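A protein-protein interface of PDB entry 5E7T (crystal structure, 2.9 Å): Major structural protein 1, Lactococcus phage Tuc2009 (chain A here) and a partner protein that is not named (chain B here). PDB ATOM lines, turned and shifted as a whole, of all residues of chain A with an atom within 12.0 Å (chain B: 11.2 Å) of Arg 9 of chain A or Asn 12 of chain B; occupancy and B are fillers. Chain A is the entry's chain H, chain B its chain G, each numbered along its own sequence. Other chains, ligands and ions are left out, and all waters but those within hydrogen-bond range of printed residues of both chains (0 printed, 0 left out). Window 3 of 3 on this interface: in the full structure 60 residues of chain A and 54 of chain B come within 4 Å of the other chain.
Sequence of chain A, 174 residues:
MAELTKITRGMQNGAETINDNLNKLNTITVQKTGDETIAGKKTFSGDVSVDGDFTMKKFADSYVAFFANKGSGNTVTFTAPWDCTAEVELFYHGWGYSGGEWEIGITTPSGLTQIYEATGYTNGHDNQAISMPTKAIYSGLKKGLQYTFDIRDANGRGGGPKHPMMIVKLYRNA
The backbone carbonyl oxygen (O) of Asn 12 of chain B is in hydrogen-bond range of the side-chain hydroxyl (OG1) of Thr 16 of chain B, at 2.7 Å. The side-chain amide nitrogen (ND2) of Asn 21 of chain A sits at hydrogen-bond distance from the backbone carbonyl oxygen (O) of Thr 5 of chain A, 2.8 Å away. The side-chain sulfur of Met 11 of chain A lies within hydrogen-bond range of the backbone NH of Thr 8 of chain A (3.6 Å). The backbone carbonyl oxygen (O) of Thr 17 of chain A sits close to the side-chain amide nitrogen (ND2) of Asn 21 of chain A.
Among the printed residues, merely in contact across the chains: Lys 6 of chain A with Asn 18 of chain B (3.6 Å), Ile 7 of chain A with Ala 14 of chain B (3.6 Å), Ile 7 of chain A with Leu 21 of chain B (3.8 Å), Thr 8 of chain A with Ala 14 of chain B (3.8 Å), Arg 9 of chain A with Asn 12 of chain B (3.5 Å), Arg 9 of chain A with Ala 14 of chain B (3.5 Å) and Asn 21 of chain A with Leu 21 of chain B (3.8 Å).
Arg 9 of chain A touches just these residues of chain B: Asn 12, Ala 14 and Glu 15. Asn 12 of chain B touches just one residue of chain A: Arg 9. Of chain B, only Ala 14 (3.8 Å) comes within 4 Å of Thr 8 of chain A. No residue of chain B comes within 4 Å of Gly 10 of chain A. No residue of chain A comes within 4 Å of Met 10 of chain B. No residue of chain A comes within 4 Å of Gln 11 of chain B. No residue of chain A comes within 4 Å of Gly 13 of chain B. Ala 14 of chain B touches just these residues of chain A: Ile 7, Thr 8 and Arg 9. Glu 15 of chain B touches just one residue of chain A: Arg 9. No residue of chain A comes within 4 Å of Thr 16 of chain B. Printed residues of chain B within 4 Å of Ile 7 of chain A: Ala 14, Asn 18 and Leu 21. Of the printed residues of chain B, Asn 21 of chain A touches Leu 21. Printed residues of chain A within 4 Å of Asn 18 of chain B: Lys 6 (3.6 Å) and Ile 7 (2.8 Å). Of the printed residues of chain B, Lys 6 of chain A touches Asn 18. Of the printed residues of chain A, Leu 21 of chain B touches Ile 7 and Asn 21. Ala 15 of chain A touches none of the printed residues of chain B. Ile 6 of chain B touches none of the printed residues of chain A. The nearest residue of chain A that does not touch Asn 12 of chain B is Ile 7 of chain A (8.2 Å).
Along chain A the printed residues that touch a printed residue of chain B span positions 6 to 21. Among the printed residues, 9 pairs touch across the chains. Among the printed residues, Asp or Glu carboxylates within 4 Å of a Lys or Arg side-chain nitrogen of the other chain: Arg 9 of chain A with Glu 15 of chain B (2.6 Å).
The side-chain carboxylate (OE1) of Glu 15 of chain B lies within salt-bridge range of the guanidinium group (NH2) of Arg 9 of chain A. N of Ile 7 of chain A is in hydrogen-bond range of OD1 of Asn 18 of chain B.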
ATOM      1  N   THR A   5      -6.219   3.457 -13.750  1.00  0.00           N
ATOM      2  CA  THR A   5      -5.657   2.253 -14.350  1.00  0.00           C
ATOM      3  C   THR A   5      -6.369   1.026 -13.728  1.00  0.00           C
ATOM      4  O   THR A   5      -6.460   0.909 -12.508  1.00  0.00           O
ATOM      5  CB  THR A   5      -4.100   2.229 -14.350  1.00  0.00           C
ATOM      6  OG1 THR A   5      -3.618   0.897 -14.133  1.00  0.00           O
ATOM      7  CG2 THR A   5      -3.462   3.232 -13.381  1.00  0.00           C
ATOM      8  N   LYS A   6      -6.908   0.145 -14.589  1.00  0.00           N
ATOM      9  CA  LYS A   6      -7.671  -1.057 -14.223  1.00  0.00           C
ATOM     10  C   LYS A   6      -6.920  -1.971 -13.290  1.00  0.00           C
ATOM     11  O   LYS A   6      -5.740  -2.255 -13.521  1.00  0.00           O
ATOM     12  CB  LYS A   6      -8.092  -1.831 -15.481  1.00  0.00           C
ATOM     13  CG  LYS A   6      -9.198  -2.852 -15.284  1.00  0.00           C
ATOM     14  CD  LYS A   6      -9.417  -3.674 -16.541  1.00  0.00           C
ATOM     15  CE  LYS A   6     -10.474  -4.726 -16.363  1.00  0.00           C
ATOM     16  NZ  LYS A   6     -10.929  -5.280 -17.668  1.00  0.00           N
ATOM     17  N   ILE A   7      -7.631  -2.424 -12.232  1.00  0.00           N
ATOM     18  CA  ILE A   7      -7.167  -3.345 -11.194  1.00  0.00           C
ATOM     19  C   ILE A   7      -7.681  -4.724 -11.569  1.00  0.00           C
ATOM     20  O   ILE A   7      -8.888  -4.964 -11.565  1.00  0.00           O
ATOM     21  CB  ILE A   7      -7.615  -2.907  -9.770  1.00  0.00           C
ATOM     22  CG1 ILE A   7      -7.141  -1.462  -9.414  1.00  0.00           C
ATOM     23  CG2 ILE A   7      -7.219  -3.918  -8.691  1.00  0.00           C
ATOM     24  CD1 ILE A   7      -5.713  -1.167  -9.549  1.00  0.00           C
ATOM     25  N   THR A   8      -6.766  -5.619 -11.937  1.00  0.00           N
ATOM     26  CA  THR A   8      -7.088  -6.979 -12.343  1.00  0.00           C
ATOM     27  C   THR A   8      -6.363  -8.005 -11.484  1.00  0.00           C
ATOM     28  O   THR A   8      -5.273  -7.712 -11.005  1.00  0.00           O
ATOM     29  CB  THR A   8      -6.753  -7.194 -13.829  1.00  0.00           C
ATOM     30  OG1 THR A   8      -5.364  -7.032 -14.055  1.00  0.00           O
ATOM     31  CG2 THR A   8      -7.502  -6.266 -14.733  1.00  0.00           C
ATOM     32  N   ARG A   9      -6.943  -9.213 -11.305  1.00  0.00           N
ATOM     33  CA  ARG A   9      -6.280 -10.306 -10.586  1.00  0.00           C
ATOM     34  C   ARG A   9      -5.045 -10.720 -11.403  1.00  0.00           C
ATOM     35  O   ARG A   9      -5.124 -10.834 -12.622  1.00  0.00           O
ATOM     36  CB  ARG A   9      -7.224 -11.497 -10.485  1.00  0.00           C
ATOM     37  CG  ARG A   9      -6.678 -12.712  -9.713  1.00  0.00           C
ATOM     38  CD  ARG A   9      -7.737 -13.795  -9.481  1.00  0.00           C
ATOM     39  NE  ARG A   9      -9.091 -13.232  -9.445  1.00  0.00           N
ATOM     40  CZ  ARG A   9      -9.712 -12.842  -8.342  1.00  0.00           C
ATOM     41  NH1 ARG A   9      -9.161 -13.043  -7.153  1.00  0.00           N
ATOM     42  NH2 ARG A   9     -10.925 -12.324  -8.410  1.00  0.00           N
ATOM     43  N   GLY A  10      -3.919 -10.886 -10.737  1.00  0.00           N
ATOM     44  CA  GLY A  10      -2.670 -11.273 -11.376  1.00  0.00           C
ATOM     45  C   GLY A  10      -1.804 -10.130 -11.863  1.00  0.00           C
ATOM     46  O   GLY A  10      -0.685 -10.368 -12.324  1.00  0.00           O
ATOM     47  N   MET A  11      -2.301  -8.886 -11.775  1.00  0.00           N
ATOM     48  CA  MET A  11      -1.550  -7.698 -12.196  1.00  0.00           C
ATOM     49  C   MET A  11      -0.261  -7.531 -11.380  1.00  0.00           C
ATOM     50  O   MET A  11      -0.189  -8.011 -10.249  1.00  0.00           O
ATOM     51  CB  MET A  11      -2.427  -6.431 -12.161  1.00  0.00           C
ATOM     52  CG  MET A  11      -2.570  -5.815 -10.794  1.00  0.00           C
ATOM     53  SD  MET A  11      -3.591  -4.364 -10.815  1.00  0.00           S
ATOM     54  CE  MET A  11      -2.620  -3.325 -11.727  1.00  0.00           C
ATOM     55  N   GLN A  12       0.719  -6.800 -11.934  1.00  0.00           N
ATOM     56  CA  GLN A  12       2.040  -6.664 -11.353  1.00  0.00           C
ATOM     57  C   GLN A  12       2.145  -5.745 -10.133  1.00  0.00           C
ATOM     58  O   GLN A  12       2.641  -6.208  -9.078  1.00  0.00           O
ATOM     59  CB  GLN A  12       3.068  -6.280 -12.399  1.00  0.00           C
ATOM     60  CG  GLN A  12       3.447  -7.460 -13.285  1.00  0.00           C
ATOM     61  CD  GLN A  12       4.918  -7.491 -13.593  1.00  0.00           C
ATOM     62  OE1 GLN A  12       5.466  -6.610 -14.291  1.00  0.00           O
ATOM     63  NE2 GLN A  12       5.587  -8.510 -13.054  1.00  0.00           N
ATOM     64  N   ASN A  13       1.755  -4.474 -10.236  1.00  0.00           N
ATOM     65  CA  ASN A  13       1.949  -3.657  -9.041  1.00  0.00           C
ATOM     66  C   ASN A  13       0.613  -3.255  -8.484  1.00  0.00           C
ATOM     67  O   ASN A  13       0.227  -2.086  -8.566  1.00  0.00           O
ATOM     68  CB  ASN A  13       2.864  -2.492  -9.344  1.00  0.00           C
ATOM     69  CG  ASN A  13       4.253  -2.919  -9.751  1.00  0.00           C
ATOM     70  OD1 ASN A  13       4.942  -3.639  -9.016  1.00  0.00           O
ATOM     71  ND2 ASN A  13       4.690  -2.493 -10.938  1.00  0.00           N
ATOM     72  N   GLY A  14      -0.102  -4.254  -7.976  1.00  0.00           N
ATOM     73  CA  GLY A  14      -1.458  -4.128  -7.474  1.00  0.00           C
ATOM     74  C   GLY A  14      -1.609  -3.084  -6.406  1.00  0.00           C
ATOM     75  O   GLY A  14      -2.414  -2.170  -6.561  1.00  0.00           O
ATOM     76  N   ALA A  15      -0.815  -3.198  -5.327  1.00  0.00           N
ATOM     77  CA  ALA A  15      -0.846  -2.274  -4.180  1.00  0.00           C
ATOM     78  C   ALA A  15      -0.554  -0.830  -4.612  1.00  0.00           C
ATOM     79  O   ALA A  15      -1.294   0.089  -4.273  1.00  0.00           O
ATOM     80  CB  ALA A  15       0.151  -2.718  -3.126  1.00  0.00           C
ATOM     81  N   THR A  17      -0.750   0.438  -7.772  1.00  0.00           N
ATOM     82  CA  THR A  17      -1.764   0.944  -8.716  1.00  0.00           C
ATOM     83  C   THR A  17      -3.022   1.338  -7.954  1.00  0.00           C
ATOM     84  O   THR A  17      -3.611   2.373  -8.290  1.00  0.00           O
ATOM     85  CB  THR A  17      -2.035  -0.035  -9.862  1.00  0.00           C
ATOM     86  OG1 THR A  17      -0.783  -0.401 -10.455  1.00  0.00           O
ATOM     87  CG2 THR A  17      -2.968   0.542 -10.927  1.00  0.00           C
ATOM     88  N   ILE A  18      -3.406   0.562  -6.891  1.00  0.00           N
ATOM     89  CA  ILE A  18      -4.553   0.899  -6.038  1.00  0.00           C
ATOM     90  C   ILE A  18      -4.238   2.233  -5.340  1.00  0.00           C
ATOM     91  O   ILE A  18      -5.087   3.125  -5.319  1.00  0.00           O
ATOM     92  CB  ILE A  18      -4.924  -0.225  -5.038  1.00  0.00           C
ATOM     93  CG1 ILE A  18      -5.437  -1.482  -5.778  1.00  0.00           C
ATOM     94  CG2 ILE A  18      -5.958   0.256  -4.014  1.00  0.00           C
ATOM     95  CD1 ILE A  18      -5.404  -2.737  -4.992  1.00  0.00           C
ATOM     96  N   ASN A  21      -4.542   5.115  -7.838  1.00  0.00           N
ATOM     97  CA  ASN A  21      -5.939   5.374  -8.193  1.00  0.00           C
ATOM     98  C   ASN A  21      -6.649   6.121  -7.065  1.00  0.00           C
ATOM     99  O   ASN A  21      -7.395   7.065  -7.339  1.00  0.00           O
ATOM    100  CB  ASN A  21      -6.673   4.089  -8.578  1.00  0.00           C
ATOM    101  CG  ASN A  21      -6.257   3.491  -9.909  1.00  0.00           C
ATOM    102  OD1 ASN A  21      -5.687   4.141 -10.790  1.00  0.00           O
ATOM    103  ND2 ASN A  21      -6.551   2.225 -10.090  1.00  0.00           N
ATOM    104  N   THR B   4     -19.340  -1.777  -2.381  1.00  0.00           N
ATOM    105  CA  THR B   4     -19.306  -3.138  -1.846  1.00  0.00           C
ATOM    106  C   THR B   4     -18.071  -3.278  -0.936  1.00  0.00           C
ATOM    107  O   THR B   4     -16.954  -2.987  -1.369  1.00  0.00           O
ATOM    108  CB  THR B   4     -19.371  -4.162  -2.996  1.00  0.00           C
ATOM    109  OG1 THR B   4     -20.544  -3.953  -3.785  1.00  0.00           O
ATOM    110  CG2 THR B   4     -19.335  -5.561  -2.523  1.00  0.00           C
ATOM    111  N   LYS B   5     -18.280  -3.703   0.327  1.00  0.00           N
ATOM    112  CA  LYS B   5     -17.223  -3.848   1.330  1.00  0.00           C
ATOM    113  C   LYS B   5     -16.086  -4.760   0.890  1.00  0.00           C
ATOM    114  O   LYS B   5     -16.331  -5.854   0.370  1.00  0.00           O
ATOM    115  CB  LYS B   5     -17.818  -4.335   2.654  1.00  0.00           C
ATOM    116  CG  LYS B   5     -16.938  -4.097   3.872  1.00  0.00           C
ATOM    117  CD  LYS B   5     -17.552  -4.705   5.112  1.00  0.00           C
ATOM    118  CE  LYS B   5     -16.672  -4.532   6.320  1.00  0.00           C
ATOM    119  NZ  LYS B   5     -17.474  -4.467   7.580  1.00  0.00           N
ATOM    120  N   ILE B   6     -14.842  -4.285   1.101  1.00  0.00           N
ATOM    121  CA  ILE B   6     -13.583  -4.988   0.825  1.00  0.00           C
ATOM    122  C   ILE B   6     -13.123  -5.564   2.159  1.00  0.00           C
ATOM    123  O   ILE B   6     -12.797  -4.802   3.077  1.00  0.00           O
ATOM    124  CB  ILE B   6     -12.506  -4.046   0.200  1.00  0.00           C
ATOM    125  CG1 ILE B   6     -13.013  -3.355  -1.091  1.00  0.00           C
ATOM    126  CG2 ILE B   6     -11.181  -4.765  -0.027  1.00  0.00           C
ATOM    127  CD1 ILE B   6     -13.537  -4.268  -2.167  1.00  0.00           C
ATOM    128  N   THR B   7     -13.131  -6.898   2.276  1.00  0.00           N
ATOM    129  CA  THR B   7     -12.734  -7.595   3.490  1.00  0.00           C
ATOM    130  C   THR B   7     -11.575  -8.571   3.260  1.00  0.00           C
ATOM    131  O   THR B   7     -11.380  -9.055   2.147  1.00  0.00           O
ATOM    132  CB  THR B   7     -13.937  -8.328   4.092  1.00  0.00           C
ATOM    133  OG1 THR B   7     -14.414  -9.319   3.178  1.00  0.00           O
ATOM    134  CG2 THR B   7     -15.037  -7.391   4.510  1.00  0.00           C
ATOM    135  N   ARG B   8     -10.839  -8.904   4.338  1.00  0.00           N
ATOM    136  CA  ARG B   8      -9.768  -9.907   4.317  1.00  0.00           C
ATOM    137  C   ARG B   8     -10.400 -11.262   4.013  1.00  0.00           C
ATOM    138  O   ARG B   8     -11.402 -11.636   4.614  1.00  0.00           O
ATOM    139  CB  ARG B   8      -9.114  -9.952   5.706  1.00  0.00           C
ATOM    140  CG  ARG B   8      -7.929 -10.862   5.870  1.00  0.00           C
ATOM    141  CD  ARG B   8      -7.243 -10.570   7.190  1.00  0.00           C
ATOM    142  NE  ARG B   8      -5.789 -10.518   7.031  1.00  0.00           N
ATOM    143  CZ  ARG B   8      -5.076  -9.400   6.930  1.00  0.00           C
ATOM    144  NH1 ARG B   8      -5.669  -8.214   7.027  1.00  0.00           N
ATOM    145  NH2 ARG B   8      -3.762  -9.457   6.759  1.00  0.00           N
ATOM    146  N   GLY B   9      -9.835 -11.970   3.063  1.00  0.00           N
ATOM    147  CA  GLY B   9     -10.309 -13.294   2.688  1.00  0.00           C
ATOM    148  C   GLY B   9     -11.400 -13.349   1.640  1.00  0.00           C
ATOM    149  O   GLY B   9     -11.800 -14.448   1.231  1.00  0.00           O
ATOM    150  N   MET B  10     -11.916 -12.189   1.226  1.00  0.00           N
ATOM    151  CA  MET B  10     -12.994 -12.116   0.255  1.00  0.00           C
ATOM    152  C   MET B  10     -12.608 -12.712  -1.080  1.00  0.00           C
ATOM    153  O   MET B  10     -11.420 -12.770  -1.461  1.00  0.00           O
ATOM    154  CB  MET B  10     -13.483 -10.658   0.057  1.00  0.00           C
ATOM    155  CG  MET B  10     -12.625  -9.832  -0.897  1.00  0.00           C
ATOM    156  SD  MET B  10     -13.220  -8.176  -1.104  1.00  0.00           S
ATOM    157  CE  MET B  10     -14.746  -8.460  -1.868  1.00  0.00           C
ATOM    158  N   GLN B  11     -13.648 -13.121  -1.788  1.00  0.00           N
ATOM    159  CA  GLN B  11     -13.568 -13.609  -3.142  1.00  0.00           C
ATOM    160  C   GLN B  11     -13.893 -12.419  -4.004  1.00  0.00           C
ATOM    161  O   GLN B  11     -14.700 -11.562  -3.624  1.00  0.00           O
ATOM    162  CB  GLN B  11     -14.584 -14.733  -3.387  1.00  0.00           C
ATOM    163  CG  GLN B  11     -14.221 -16.053  -2.721  1.00  0.00           C
ATOM    164  CD  GLN B  11     -12.856 -16.568  -3.076  1.00  0.00           C
ATOM    165  OE1 GLN B  11     -12.553 -16.879  -4.232  1.00  0.00           O
ATOM    166  NE2 GLN B  11     -12.000 -16.653  -2.084  1.00  0.00           N
ATOM    167  N   ASN B  12     -13.269 -12.374  -5.163  1.00  0.00           N
ATOM    168  CA  ASN B  12     -13.440 -11.336  -6.169  1.00  0.00           C
ATOM    169  C   ASN B  12     -12.952  -9.986  -5.700  1.00  0.00           C
ATOM    170  O   ASN B  12     -13.542  -8.958  -6.047  1.00  0.00           O
ATOM    171  CB  ASN B  12     -14.875 -11.287  -6.672  1.00  0.00           C
ATOM    172  CG  ASN B  12     -15.409 -12.631  -7.133  1.00  0.00           C
ATOM    173  OD1 ASN B  12     -14.802 -13.340  -7.969  1.00  0.00           O
ATOM    174  ND2 ASN B  12     -16.583 -12.977  -6.618  1.00  0.00           N
ATOM    175  N   GLY B  13     -11.844 -10.006  -4.954  1.00  0.00           N
ATOM    176  CA  GLY B  13     -11.200  -8.827  -4.387  1.00  0.00           C
ATOM    177  C   GLY B  13     -10.806  -7.812  -5.431  1.00  0.00           C
ATOM    178  O   GLY B  13     -11.186  -6.656  -5.307  1.00  0.00           O
ATOM    179  N   ALA B  14     -10.074  -8.238  -6.488  1.00  0.00           N
ATOM    180  CA  ALA B  14      -9.605  -7.368  -7.551  1.00  0.00           C
ATOM    181  C   ALA B  14     -10.752  -6.703  -8.276  1.00  0.00           C
ATOM    182  O   ALA B  14     -10.733  -5.486  -8.467  1.00  0.00           O
ATOM    183  CB  ALA B  14      -8.738  -8.133  -8.524  1.00  0.00           C
ATOM    184  N   GLU B  15     -11.784  -7.463  -8.623  1.00  0.00           N
ATOM    185  CA  GLU B  15     -12.940  -6.914  -9.349  1.00  0.00           C
ATOM    186  C   GLU B  15     -13.758  -5.992  -8.478  1.00  0.00           C
ATOM    187  O   GLU B  15     -14.165  -4.934  -8.965  1.00  0.00           O
ATOM    188  CB  GLU B  15     -13.822  -8.011  -9.933  1.00  0.00           C
ATOM    189  CG  GLU B  15     -13.052  -8.994 -10.784  1.00  0.00           C
ATOM    190  CD  GLU B  15     -12.541 -10.212 -10.064  1.00  0.00           C
ATOM    191  OE1 GLU B  15     -12.224 -10.111  -8.858  1.00  0.00           O
ATOM    192  OE2 GLU B  15     -12.485 -11.285 -10.703  1.00  0.00           O
ATOM    193  N   THR B  16     -13.973  -6.366  -7.179  1.00  0.00           N
ATOM    194  CA  THR B  16     -14.741  -5.511  -6.281  1.00  0.00           C
ATOM    195  C   THR B  16     -14.011  -4.194  -6.065  1.00  0.00           C
ATOM    196  O   THR B  16     -14.661  -3.151  -6.099  1.00  0.00           O
ATOM    197  CB  THR B  16     -15.133  -6.239  -5.003  1.00  0.00           C
ATOM    198  OG1 THR B  16     -15.714  -7.517  -5.304  1.00  0.00           O
ATOM    199  CG2 THR B  16     -16.110  -5.468  -4.199  1.00  0.00           C
ATOM    200  N   ILE B  17     -12.658  -4.220  -5.928  1.00  0.00           N
ATOM    201  CA  ILE B  17     -11.846  -2.994  -5.787  1.00  0.00           C
ATOM    202  C   ILE B  17     -11.998  -2.164  -7.081  1.00  0.00           C
ATOM    203  O   ILE B  17     -12.246  -0.955  -7.020  1.00  0.00           O
ATOM    204  CB  ILE B  17     -10.358  -3.272  -5.422  1.00  0.00           C
ATOM    205  CG1 ILE B  17     -10.234  -3.908  -4.038  1.00  0.00           C
ATOM    206  CG2 ILE B  17      -9.531  -1.977  -5.460  1.00  0.00           C
ATOM    207  CD1 ILE B  17      -8.944  -4.585  -3.787  1.00  0.00           C
ATOM    208  N   ASN B  18     -11.921  -2.837  -8.242  1.00  0.00           N
ATOM    209  CA  ASN B  18     -12.043  -2.178  -9.537  1.00  0.00           C
ATOM    210  C   ASN B  18     -13.380  -1.509  -9.694  1.00  0.00           C
ATOM    211  O   ASN B  18     -13.425  -0.355 -10.099  1.00  0.00           O
ATOM    212  CB  ASN B  18     -11.827  -3.166 -10.669  1.00  0.00           C
ATOM    213  CG  ASN B  18     -11.365  -2.524 -11.924  1.00  0.00           C
ATOM    214  OD1 ASN B  18     -10.338  -1.855 -11.951  1.00  0.00           O
ATOM    215  ND2 ASN B  18     -12.069  -2.775 -13.010  1.00  0.00           N
ATOM    216  N   ASP B  19     -14.467  -2.219  -9.350  1.00  0.00           N
ATOM    217  CA  ASP B  19     -15.826  -1.708  -9.469  1.00  0.00           C
ATOM    218  C   ASP B  19     -16.009  -0.513  -8.548  1.00  0.00           C
ATOM    219  O   ASP B  19     -16.600   0.484  -8.964  1.00  0.00           O
ATOM    220  CB  ASP B  19     -16.868  -2.801  -9.165  1.00  0.00           C
ATOM    221  CG  ASP B  19     -16.981  -3.952 -10.160  1.00  0.00           C
ATOM    222  OD1 ASP B  19     -16.435  -3.828 -11.277  1.00  0.00           O
ATOM    223  OD2 ASP B  19     -17.675  -4.960  -9.835  1.00  0.00           O
ATOM    224  N   ASN B  20     -15.465  -0.596  -7.323  1.00  0.00           N
ATOM    225  CA  ASN B  20     -15.575   0.488  -6.349  1.00  0.00           C
ATOM    226  C   ASN B  20     -14.831   1.757  -6.785  1.00  0.00           C
ATOM    227  O   ASN B  20     -15.368   2.862  -6.645  1.00  0.00           O
ATOM    228  CB  ASN B  20     -15.163   0.018  -4.969  1.00  0.00           C
ATOM    229  CG  ASN B  20     -16.112  -0.988  -4.360  1.00  0.00           C
ATOM    230  OD1 ASN B  20     -17.239  -1.221  -4.811  1.00  0.00           O
ATOM    231  ND2 ASN B  20     -15.680  -1.612  -3.313  1.00  0.00           N
ATOM    232  N   LEU B  21     -13.632   1.588  -7.380  1.00  0.00           N
ATOM    233  CA  LEU B  21     -12.847   2.686  -7.912  1.00  0.00           C
ATOM    234  C   LEU B  21     -13.589   3.285  -9.102  1.00  0.00           C
ATOM    235  O   LEU B  21     -13.695   4.511  -9.204  1.00  0.00           O
ATOM    236  CB  LEU B  21     -11.469   2.193  -8.334  1.00  0.00           C
ATOM    237  CG  LEU B  21     -10.481   1.880  -7.216  1.00  0.00           C
ATOM    238  CD1 LEU B  21      -9.315   1.123  -7.759  1.00  0.00           C
ATOM    239  CD2 LEU B  21     -10.000   3.149  -6.519  1.00  0.00           C
ATOM    240  N   LYS B  23     -16.914   3.125  -9.611  1.00  0.00           N
ATOM    241  CA  LYS B  23     -18.141   3.731  -9.069  1.00  0.00           C
ATOM    242  C   LYS B  23     -17.818   5.119  -8.620  1.00  0.00           C
ATOM    243  O   LYS B  23     -18.432   6.057  -9.119  1.00  0.00           O
ATOM    244  CB  LYS B  23     -18.720   2.919  -7.894  1.00  0.00           C
ATOM    245  CG  LYS B  23     -20.231   2.643  -8.016  1.00  0.00           C
ATOM    246  CD  LYS B  23     -20.729   1.532  -7.049  1.00  0.00           C
ATOM    247  CE  LYS B  23     -20.566   0.109  -7.553  1.00  0.00           C
ATOM    248  NZ  LYS B  23     -20.433  -0.862  -6.431  1.00  0.00           N
